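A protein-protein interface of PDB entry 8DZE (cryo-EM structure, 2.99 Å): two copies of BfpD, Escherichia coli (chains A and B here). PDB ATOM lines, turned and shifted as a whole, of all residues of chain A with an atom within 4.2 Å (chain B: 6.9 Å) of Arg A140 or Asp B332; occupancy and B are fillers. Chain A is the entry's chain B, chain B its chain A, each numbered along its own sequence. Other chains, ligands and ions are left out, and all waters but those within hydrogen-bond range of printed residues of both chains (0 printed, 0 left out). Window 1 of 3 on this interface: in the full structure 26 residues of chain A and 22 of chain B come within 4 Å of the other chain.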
ATOM      1  N   VAL A 123      14.002  28.903 -17.500  1.00  0.00           N
ATOM      2  CA  VAL A 123      12.721  28.600 -18.112  1.00  0.00           C
ATOM      3  C   VAL A 123      12.265  27.234 -17.621  1.00  0.00           C
ATOM      4  O   VAL A 123      13.052  26.423 -17.125  1.00  0.00           O
ATOM      5  CB  VAL A 123      12.790  28.648 -19.657  1.00  0.00           C
ATOM      6  CG1 VAL A 123      13.600  29.848 -20.114  1.00  0.00           C
ATOM      7  CG2 VAL A 123      13.380  27.360 -20.213  1.00  0.00           C
ATOM      8  N   SER A 124      10.963  26.977 -17.741  1.00  0.00           N
ATOM      9  CA  SER A 124      10.410  25.704 -17.287  1.00  0.00           C
ATOM     10  C   SER A 124      10.388  24.670 -18.410  1.00  0.00           C
ATOM     11  O   SER A 124      11.081  23.652 -18.338  1.00  0.00           O
ATOM     12  CB  SER A 124       9.002  25.915 -16.720  1.00  0.00           C
ATOM     13  OG  SER A 124       9.033  26.749 -15.575  1.00  0.00           O
ATOM     14  N   ASP A 125       9.611  24.928 -19.460  1.00  0.00           N
ATOM     15  CA  ASP A 125       9.513  24.034 -20.603  1.00  0.00           C
ATOM     16  C   ASP A 125      10.079  24.719 -21.841  1.00  0.00           C
ATOM     17  O   ASP A 125      10.114  25.949 -21.935  1.00  0.00           O
ATOM     18  CB  ASP A 125       8.063  23.600 -20.886  1.00  0.00           C
ATOM     19  CG  ASP A 125       7.348  23.051 -19.659  1.00  0.00           C
ATOM     20  OD1 ASP A 125       6.363  22.306 -19.841  1.00  0.00           O
ATOM     21  OD2 ASP A 125       7.744  23.365 -18.520  1.00  0.00           O
ATOM     22  N   ILE A 139       9.753  29.448 -25.091  1.00  0.00           N
ATOM     23  CA  ILE A 139      10.117  29.109 -23.723  1.00  0.00           C
ATOM     24  C   ILE A 139       8.941  29.422 -22.811  1.00  0.00           C
ATOM     25  O   ILE A 139       8.124  30.303 -23.097  1.00  0.00           O
ATOM     26  CB  ILE A 139      11.380  29.862 -23.256  1.00  0.00           C
ATOM     27  CG1 ILE A 139      11.193  31.367 -23.441  1.00  0.00           C
ATOM     28  CG2 ILE A 139      12.605  29.367 -24.004  1.00  0.00           C
ATOM     29  CD1 ILE A 139      12.283  32.196 -22.825  1.00  0.00           C
ATOM     30  N   ARG A 140       8.853  28.683 -21.710  1.00  0.00           N
ATOM     31  CA  ARG A 140       7.831  28.900 -20.689  1.00  0.00           C
ATOM     32  C   ARG A 140       8.517  29.489 -19.459  1.00  0.00           C
ATOM     33  O   ARG A 140       9.006  28.761 -18.594  1.00  0.00           O
ATOM     34  CB  ARG A 140       7.094  27.606 -20.356  1.00  0.00           C
ATOM     35  CG  ARG A 140       5.776  27.828 -19.631  1.00  0.00           C
ATOM     36  CD  ARG A 140       4.966  26.548 -19.530  1.00  0.00           C
ATOM     37  NE  ARG A 140       4.106  26.358 -20.692  1.00  0.00           N
ATOM     38  CZ  ARG A 140       2.812  26.077 -20.628  1.00  0.00           C
ATOM     39  NH1 ARG A 140       2.191  25.945 -19.468  1.00  0.00           N
ATOM     40  NH2 ARG A 140       2.125  25.924 -21.756  1.00  0.00           N
ATOM     41  N   LYS A 141       8.546  30.815 -19.389  1.00  0.00           N
ATOM     42  CA  LYS A 141       9.088  31.529 -18.242  1.00  0.00           C
ATOM     43  C   LYS A 141       7.946  31.894 -17.305  1.00  0.00           C
ATOM     44  O   LYS A 141       6.968  32.519 -17.732  1.00  0.00           O
ATOM     45  CB  LYS A 141       9.840  32.785 -18.682  1.00  0.00           C
ATOM     46  CG  LYS A 141      11.349  32.620 -18.732  1.00  0.00           C
ATOM     47  CD  LYS A 141      12.055  33.952 -18.537  1.00  0.00           C
ATOM     48  CE  LYS A 141      11.973  34.417 -17.093  1.00  0.00           C
ATOM     49  NZ  LYS A 141      12.450  33.373 -16.146  1.00  0.00           N
ATOM     50  N   ASP A 142       8.083  31.510 -16.036  1.00  0.00           N
ATOM     51  CA  ASP A 142       7.042  31.648 -15.005  1.00  0.00           C
ATOM     52  C   ASP A 142       5.809  30.898 -15.507  1.00  0.00           C
ATOM     53  O   ASP A 142       5.928  29.716 -15.870  1.00  0.00           O
ATOM     54  CB  ASP A 142       6.832  33.122 -14.666  1.00  0.00           C
ATOM     55  CG  ASP A 142       8.010  33.722 -13.925  1.00  0.00           C
ATOM     56  OD1 ASP A 142       9.025  33.017 -13.750  1.00  0.00           O
ATOM     57  OD2 ASP A 142       7.921  34.899 -13.518  1.00  0.00           O
ATOM     58  N   ASP A 144       3.677  32.033 -18.115  1.00  0.00           N
ATOM     59  CA  ASP A 144       3.284  32.446 -19.453  1.00  0.00           C
ATOM     60  C   ASP A 144       4.340  32.028 -20.467  1.00  0.00           C
ATOM     61  O   ASP A 144       5.533  31.965 -20.158  1.00  0.00           O
ATOM     62  CB  ASP A 144       3.070  33.963 -19.523  1.00  0.00           C
ATOM     63  CG  ASP A 144       2.112  34.466 -18.461  1.00  0.00           C
ATOM     64  OD1 ASP A 144       1.134  33.751 -18.156  1.00  0.00           O
ATOM     65  OD2 ASP A 144       2.337  35.574 -17.933  1.00  0.00           O
ATOM     66  N   MET A 145       3.888  31.743 -21.683  1.00  0.00           N
ATOM     67  CA  MET A 145       4.768  31.361 -22.777  1.00  0.00           C
ATOM     68  C   MET A 145       5.121  32.580 -23.619  1.00  0.00           C
ATOM     69  O   MET A 145       4.324  33.510 -23.766  1.00  0.00           O
ATOM     70  CB  MET A 145       4.115  30.294 -23.657  1.00  0.00           C
ATOM     71  CG  MET A 145       4.237  28.881 -23.117  1.00  0.00           C
ATOM     72  SD  MET A 145       4.748  27.700 -24.377  1.00  0.00           S
ATOM     73  CE  MET A 145       3.526  28.013 -25.647  1.00  0.00           C
ATOM     74  N   PRO B 252     -10.470  29.489 -17.403  1.00  0.00           N
ATOM     75  CA  PRO B 252      -9.256  28.728 -17.728  1.00  0.00           C
ATOM     76  C   PRO B 252      -9.424  27.218 -17.640  1.00  0.00           C
ATOM     77  O   PRO B 252      -8.748  26.478 -18.361  1.00  0.00           O
ATOM     78  CB  PRO B 252      -8.249  29.232 -16.687  1.00  0.00           C
ATOM     79  CG  PRO B 252      -9.097  29.591 -15.517  1.00  0.00           C
ATOM     80  CD  PRO B 252     -10.372  30.151 -16.090  1.00  0.00           C
ATOM     81  N   LYS B 284      -0.141  33.635 -24.981  1.00  0.00           N
ATOM     82  CA  LYS B 284       0.462  33.358 -23.683  1.00  0.00           C
ATOM     83  C   LYS B 284       0.201  31.940 -23.197  1.00  0.00           C
ATOM     84  O   LYS B 284       0.675  31.574 -22.117  1.00  0.00           O
ATOM     85  CB  LYS B 284      -0.043  34.357 -22.637  1.00  0.00           C
ATOM     86  CG  LYS B 284       0.546  35.750 -22.771  1.00  0.00           C
ATOM     87  CD  LYS B 284      -0.130  36.725 -21.822  1.00  0.00           C
ATOM     88  CE  LYS B 284       0.373  38.143 -22.036  1.00  0.00           C
ATOM     89  NZ  LYS B 284      -0.667  39.157 -21.707  1.00  0.00           N
ATOM     90  N   VAL B 285      -0.539  31.134 -23.959  1.00  0.00           N
ATOM     91  CA  VAL B 285      -0.854  29.765 -23.582  1.00  0.00           C
ATOM     92  C   VAL B 285      -0.528  28.845 -24.749  1.00  0.00           C
ATOM     93  O   VAL B 285      -0.437  29.270 -25.904  1.00  0.00           O
ATOM     94  CB  VAL B 285      -2.329  29.591 -23.162  1.00  0.00           C
ATOM     95  CG1 VAL B 285      -2.600  30.304 -21.846  1.00  0.00           C
ATOM     96  CG2 VAL B 285      -3.255  30.102 -24.254  1.00  0.00           C
ATOM     97  N   ASN B 286      -0.350  27.566 -24.432  1.00  0.00           N
ATOM     98  CA  ASN B 286      -0.079  26.547 -25.436  1.00  0.00           C
ATOM     99  C   ASN B 286      -1.390  25.920 -25.887  1.00  0.00           C
ATOM    100  O   ASN B 286      -2.219  25.537 -25.057  1.00  0.00           O
ATOM    101  CB  ASN B 286       0.859  25.476 -24.878  1.00  0.00           C
ATOM    102  CG  ASN B 286       1.479  24.622 -25.964  1.00  0.00           C
ATOM    103  OD1 ASN B 286       1.286  24.871 -27.153  1.00  0.00           O
ATOM    104  ND2 ASN B 286       2.229  23.604 -25.560  1.00  0.00           N
ATOM    105  N   ILE B 287      -1.580  25.828 -27.200  1.00  0.00           N
ATOM    106  CA  ILE B 287      -2.774  25.234 -27.787  1.00  0.00           C
ATOM    107  C   ILE B 287      -2.345  24.068 -28.667  1.00  0.00           C
ATOM    108  O   ILE B 287      -1.449  24.214 -29.506  1.00  0.00           O
ATOM    109  CB  ILE B 287      -3.590  26.259 -28.594  1.00  0.00           C
ATOM    110  CG1 ILE B 287      -3.841  27.520 -27.761  1.00  0.00           C
ATOM    111  CG2 ILE B 287      -4.905  25.647 -29.054  1.00  0.00           C
ATOM    112  CD1 ILE B 287      -4.838  28.479 -28.375  1.00  0.00           C
ATOM    113  N   ILE B 288      -2.979  22.917 -28.466  1.00  0.00           N
ATOM    114  CA  ILE B 288      -2.728  21.713 -29.246  1.00  0.00           C
ATOM    115  C   ILE B 288      -4.028  21.340 -29.945  1.00  0.00           C
ATOM    116  O   ILE B 288      -5.112  21.527 -29.385  1.00  0.00           O
ATOM    117  CB  ILE B 288      -2.215  20.561 -28.355  1.00  0.00           C
ATOM    118  CG1 ILE B 288      -0.928  20.975 -27.643  1.00  0.00           C
ATOM    119  CG2 ILE B 288      -1.958  19.300 -29.165  1.00  0.00           C
ATOM    120  CD1 ILE B 288      -0.461  19.984 -26.606  1.00  0.00           C
ATOM    121  N   ALA B 326      -0.168  14.066 -26.483  1.00  0.00           N
ATOM    122  CA  ALA B 326      -0.501  15.458 -26.202  1.00  0.00           C
ATOM    123  C   ALA B 326      -0.665  15.702 -24.708  1.00  0.00           C
ATOM    124  O   ALA B 326      -0.329  16.785 -24.216  1.00  0.00           O
ATOM    125  CB  ALA B 326      -1.773  15.858 -26.949  1.00  0.00           C
ATOM    126  N   SER B 329       2.837  16.151 -22.761  1.00  0.00           N
ATOM    127  CA  SER B 329       3.337  17.518 -22.757  1.00  0.00           C
ATOM    128  C   SER B 329       2.390  18.399 -21.942  1.00  0.00           C
ATOM    129  O   SER B 329       1.474  17.916 -21.272  1.00  0.00           O
ATOM    130  CB  SER B 329       3.505  18.026 -24.187  1.00  0.00           C
ATOM    131  OG  SER B 329       2.254  18.118 -24.846  1.00  0.00           O
ATOM    132  N   ASP B 330       2.610  19.713 -21.979  1.00  0.00           N
ATOM    133  CA  ASP B 330       1.725  20.653 -21.300  1.00  0.00           C
ATOM    134  C   ASP B 330       0.654  21.140 -22.269  1.00  0.00           C
ATOM    135  O   ASP B 330       0.929  21.983 -23.131  1.00  0.00           O
ATOM    136  CB  ASP B 330       2.518  21.829 -20.729  1.00  0.00           C
ATOM    137  CG  ASP B 330       3.603  22.309 -21.669  1.00  0.00           C
ATOM    138  OD1 ASP B 330       3.864  21.616 -22.674  1.00  0.00           O
ATOM    139  OD2 ASP B 330       4.190  23.380 -21.407  1.00  0.00           O
ATOM    140  N   PRO B 331      -0.576  20.635 -22.163  1.00  0.00           N
ATOM    141  CA  PRO B 331      -1.586  20.945 -23.181  1.00  0.00           C
ATOM    142  C   PRO B 331      -2.275  22.289 -23.000  1.00  0.00           C
ATOM    143  O   PRO B 331      -2.621  22.931 -23.998  1.00  0.00           O
ATOM    144  CB  PRO B 331      -2.577  19.786 -23.037  1.00  0.00           C
ATOM    145  CG  PRO B 331      -2.492  19.401 -21.594  1.00  0.00           C
ATOM    146  CD  PRO B 331      -1.112  19.770 -21.097  1.00  0.00           C
ATOM    147  N   ASP B 332      -2.484  22.715 -21.748  1.00  0.00           N
ATOM    148  CA  ASP B 332      -3.287  23.889 -21.401  1.00  0.00           C
ATOM    149  C   ASP B 332      -4.688  23.792 -22.000  1.00  0.00           C
ATOM    150  O   ASP B 332      -5.655  23.515 -21.284  1.00  0.00           O
ATOM    151  CB  ASP B 332      -2.599  25.185 -21.843  1.00  0.00           C
ATOM    152  CG  ASP B 332      -1.530  25.636 -20.870  1.00  0.00           C
ATOM    153  OD1 ASP B 332      -1.644  25.317 -19.669  1.00  0.00           O
ATOM    154  OD2 ASP B 332      -0.574  26.314 -21.305  1.00  0.00           O
ATOM    155  N   ILE B 333      -4.806  24.020 -23.306  1.00  0.00           N
ATOM    156  CA  ILE B 333      -6.044  23.801 -24.047  1.00  0.00           C
ATOM    157  C   ILE B 333      -5.815  22.614 -24.973  1.00  0.00           C
ATOM    158  O   ILE B 333      -4.890  22.628 -25.795  1.00  0.00           O
ATOM    159  CB  ILE B 333      -6.465  25.050 -24.835  1.00  0.00           C
ATOM    160  CG1 ILE B 333      -6.516  26.267 -23.910  1.00  0.00           C
ATOM    161  CG2 ILE B 333      -7.813  24.829 -25.499  1.00  0.00           C
ATOM    162  CD1 ILE B 333      -6.634  27.584 -24.640  1.00  0.00           C
ATOM    163  N   ILE B 334      -6.655  21.591 -24.845  1.00  0.00           N
ATOM    164  CA  ILE B 334      -6.398  20.317 -25.513  1.00  0.00           C
ATOM    165  C   ILE B 334      -7.033  20.265 -26.898  1.00  0.00           C
ATOM    166  O   ILE B 334      -6.428  19.727 -27.830  1.00  0.00           O
ATOM    167  CB  ILE B 334      -6.885  19.160 -24.619  1.00  0.00           C
ATOM    168  CG1 ILE B 334      -6.195  19.233 -23.259  1.00  0.00           C
ATOM    169  CG2 ILE B 334      -6.600  17.814 -25.268  1.00  0.00           C
ATOM    170  CD1 ILE B 334      -6.678  18.204 -22.282  1.00  0.00           C
ATOM    171  N   MET B 335      -8.238  20.813 -27.042  1.00  0.00           N
ATOM    172  CA  MET B 335      -8.947  20.899 -28.316  1.00  0.00           C
ATOM    173  C   MET B 335      -9.008  19.582 -29.097  1.00  0.00           C
ATOM    174  O   MET B 335      -8.475  19.489 -30.208  1.00  0.00           O
ATOM    175  CB  MET B 335      -8.339  21.997 -29.178  1.00  0.00           C
ATOM    176  CG  MET B 335      -8.823  23.398 -28.852  1.00  0.00           C
ATOM    177  SD  MET B 335     -10.336  23.826 -29.733  1.00  0.00           S
ATOM    178  CE  MET B 335     -10.327  25.609 -29.577  1.00  0.00           C
ATOM    179  N   GLY B 355      -6.766  19.865 -14.741  1.00  0.00           N
ATOM    180  CA  GLY B 355      -6.563  21.300 -14.740  1.00  0.00           C
ATOM    181  C   GLY B 355      -6.425  21.923 -16.115  1.00  0.00           C
ATOM    182  O   GLY B 355      -6.063  23.098 -16.233  1.00  0.00           O
ATOM    183  N   HIS B 356      -6.705  21.153 -17.160  1.00  0.00           N
ATOM    184  CA  HIS B 356      -6.660  21.642 -18.530  1.00  0.00           C
ATOM    185  C   HIS B 356      -8.053  22.049 -18.998  1.00  0.00           C
ATOM    186  O   HIS B 356      -9.050  21.888 -18.292  1.00  0.00           O
ATOM    187  CB  HIS B 356      -6.072  20.578 -19.461  1.00  0.00           C
ATOM    188  CG  HIS B 356      -4.855  19.900 -18.913  1.00  0.00           C
ATOM    189  ND1 HIS B 356      -3.770  20.598 -18.427  1.00  0.00           N
ATOM    190  CD2 HIS B 356      -4.551  18.589 -18.776  1.00  0.00           C
ATOM    191  CE1 HIS B 356      -2.851  19.744 -18.012  1.00  0.00           C
ATOM    192  NE2 HIS B 356      -3.299  18.519 -18.213  1.00  0.00           N
ATOM    193  N   GLN B 357      -8.110  22.588 -20.214  1.00  0.00           N
ATOM    194  CA  GLN B 357      -9.359  23.002 -20.842  1.00  0.00           C
ATOM    195  C   GLN B 357      -9.584  22.173 -22.098  1.00  0.00           C
ATOM    196  O   GLN B 357      -8.663  21.996 -22.902  1.00  0.00           O
ATOM    197  CB  GLN B 357      -9.339  24.495 -21.181  1.00  0.00           C
ATOM    198  CG  GLN B 357     -10.637  25.006 -21.780  1.00  0.00           C
ATOM    199  CD  GLN B 357     -10.801  26.504 -21.630  1.00  0.00           C
ATOM    200  OE1 GLN B 357      -9.928  27.279 -22.020  1.00  0.00           O
ATOM    201  NE2 GLN B 357     -11.927  26.922 -21.064  1.00  0.00           N
ATOM    202  N   VAL B 358     -10.804  21.666 -22.263  1.00  0.00           N
ATOM    203  CA  VAL B 358     -11.148  20.753 -23.346  1.00  0.00           C
ATOM    204  C   VAL B 358     -12.296  21.351 -24.148  1.00  0.00           C
ATOM    205  O   VAL B 358     -13.316  21.753 -23.576  1.00  0.00           O
ATOM    206  CB  VAL B 358     -11.528  19.361 -22.807  1.00  0.00           C
ATOM    207  CG1 VAL B 358     -12.060  18.475 -23.922  1.00  0.00           C
ATOM    208  CG2 VAL B 358     -10.337  18.710 -22.127  1.00  0.00           C
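The backbone NH (N) of Met A145 is in hydrogen-bond range of the backbone carbonyl oxygen (O) of Lys B284 (3.2 Å).
The guanidinium group of Arg A140 lies within salt-bridge range of the side-chain carboxylate of Asp B330 (3.1 Å).
NH2 of Arg A140 lies within salt-bridge range of OD2 of Asp B332, at 2.8 Å.
The side-chain carboxylate of Asp A125 lies close to the side-chain carboxylate of Asp B330.
The backbone carbonyl oxygen (O) of Asp B330 sits at hydrogen-bond distance from the side-chain amide nitrogen (ND2) of Asn B286 (3.2 Å).
N of Asn B286 lies within hydrogen-bond range of OD2 of Asp B332 (3.4 Å).
The backbone carbonyl oxygen (O) of Asn B286 lies within hydrogen-bond range of the backbone NH (N) of Ile B333 (3.5 Å).
O of Asp B332 sits at hydrogen-bond distance from N of Gln B357 (2.8 Å).
The backbone NH of Ser A124 is in hydrogen-bond range of the backbone carbonyl oxygen of Arg A140.
The backbone NH (N) of Arg A140 lies within hydrogen-bond range of the backbone carbonyl oxygen (O) of Asp A125.
Among the printed residues, merely in contact across the chains: Arg A140 with Asn B286, Met A145 with Asn B286 and Asp A144 with Lys B284.
Arg A140 touches just these residues of chain B: Asn B286, Asp B330 and Asp B332.
Printed residues of chain B within 4 Å of Asp A144: Lys B284 (3.8 Å).
Of the printed residues of chain B, Met A145 touches Lys B284 and Asn B286.
Of the printed residues of chain A, Lys B284 touches Asp A144 and Met A145.
Printed residues of chain A within 4 Å of Asn B286: Arg A140 (3.4 Å) and Met A145 (3.8 Å).
Of the printed residues of chain A, Asp B330 touches Asp A125 and Arg A140.
Asp B332 touches just one residue of chain A: Arg A140 (2.8 Å).
The nearest residue of chain B that does not touch Arg A140 is Val B285 (5.0 Å).
The nearest printed residue of chain A that does not touch Asp B332 is Met A145 (5.7 Å).
Of the 18 printed residues of chain B, 4 touch a printed residue of chain A.
Printed residues of chain B that touch a printed residue of chain A: Lys B284, Asn B286, Asp B330 and Asp B332.
Among the printed residues, 7 pairs touch across the chains.
No position is printed for both chains.
Of the 7 pairs that touch across the chains among the printed residues, none has its exchanged pair printed and touching as well.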
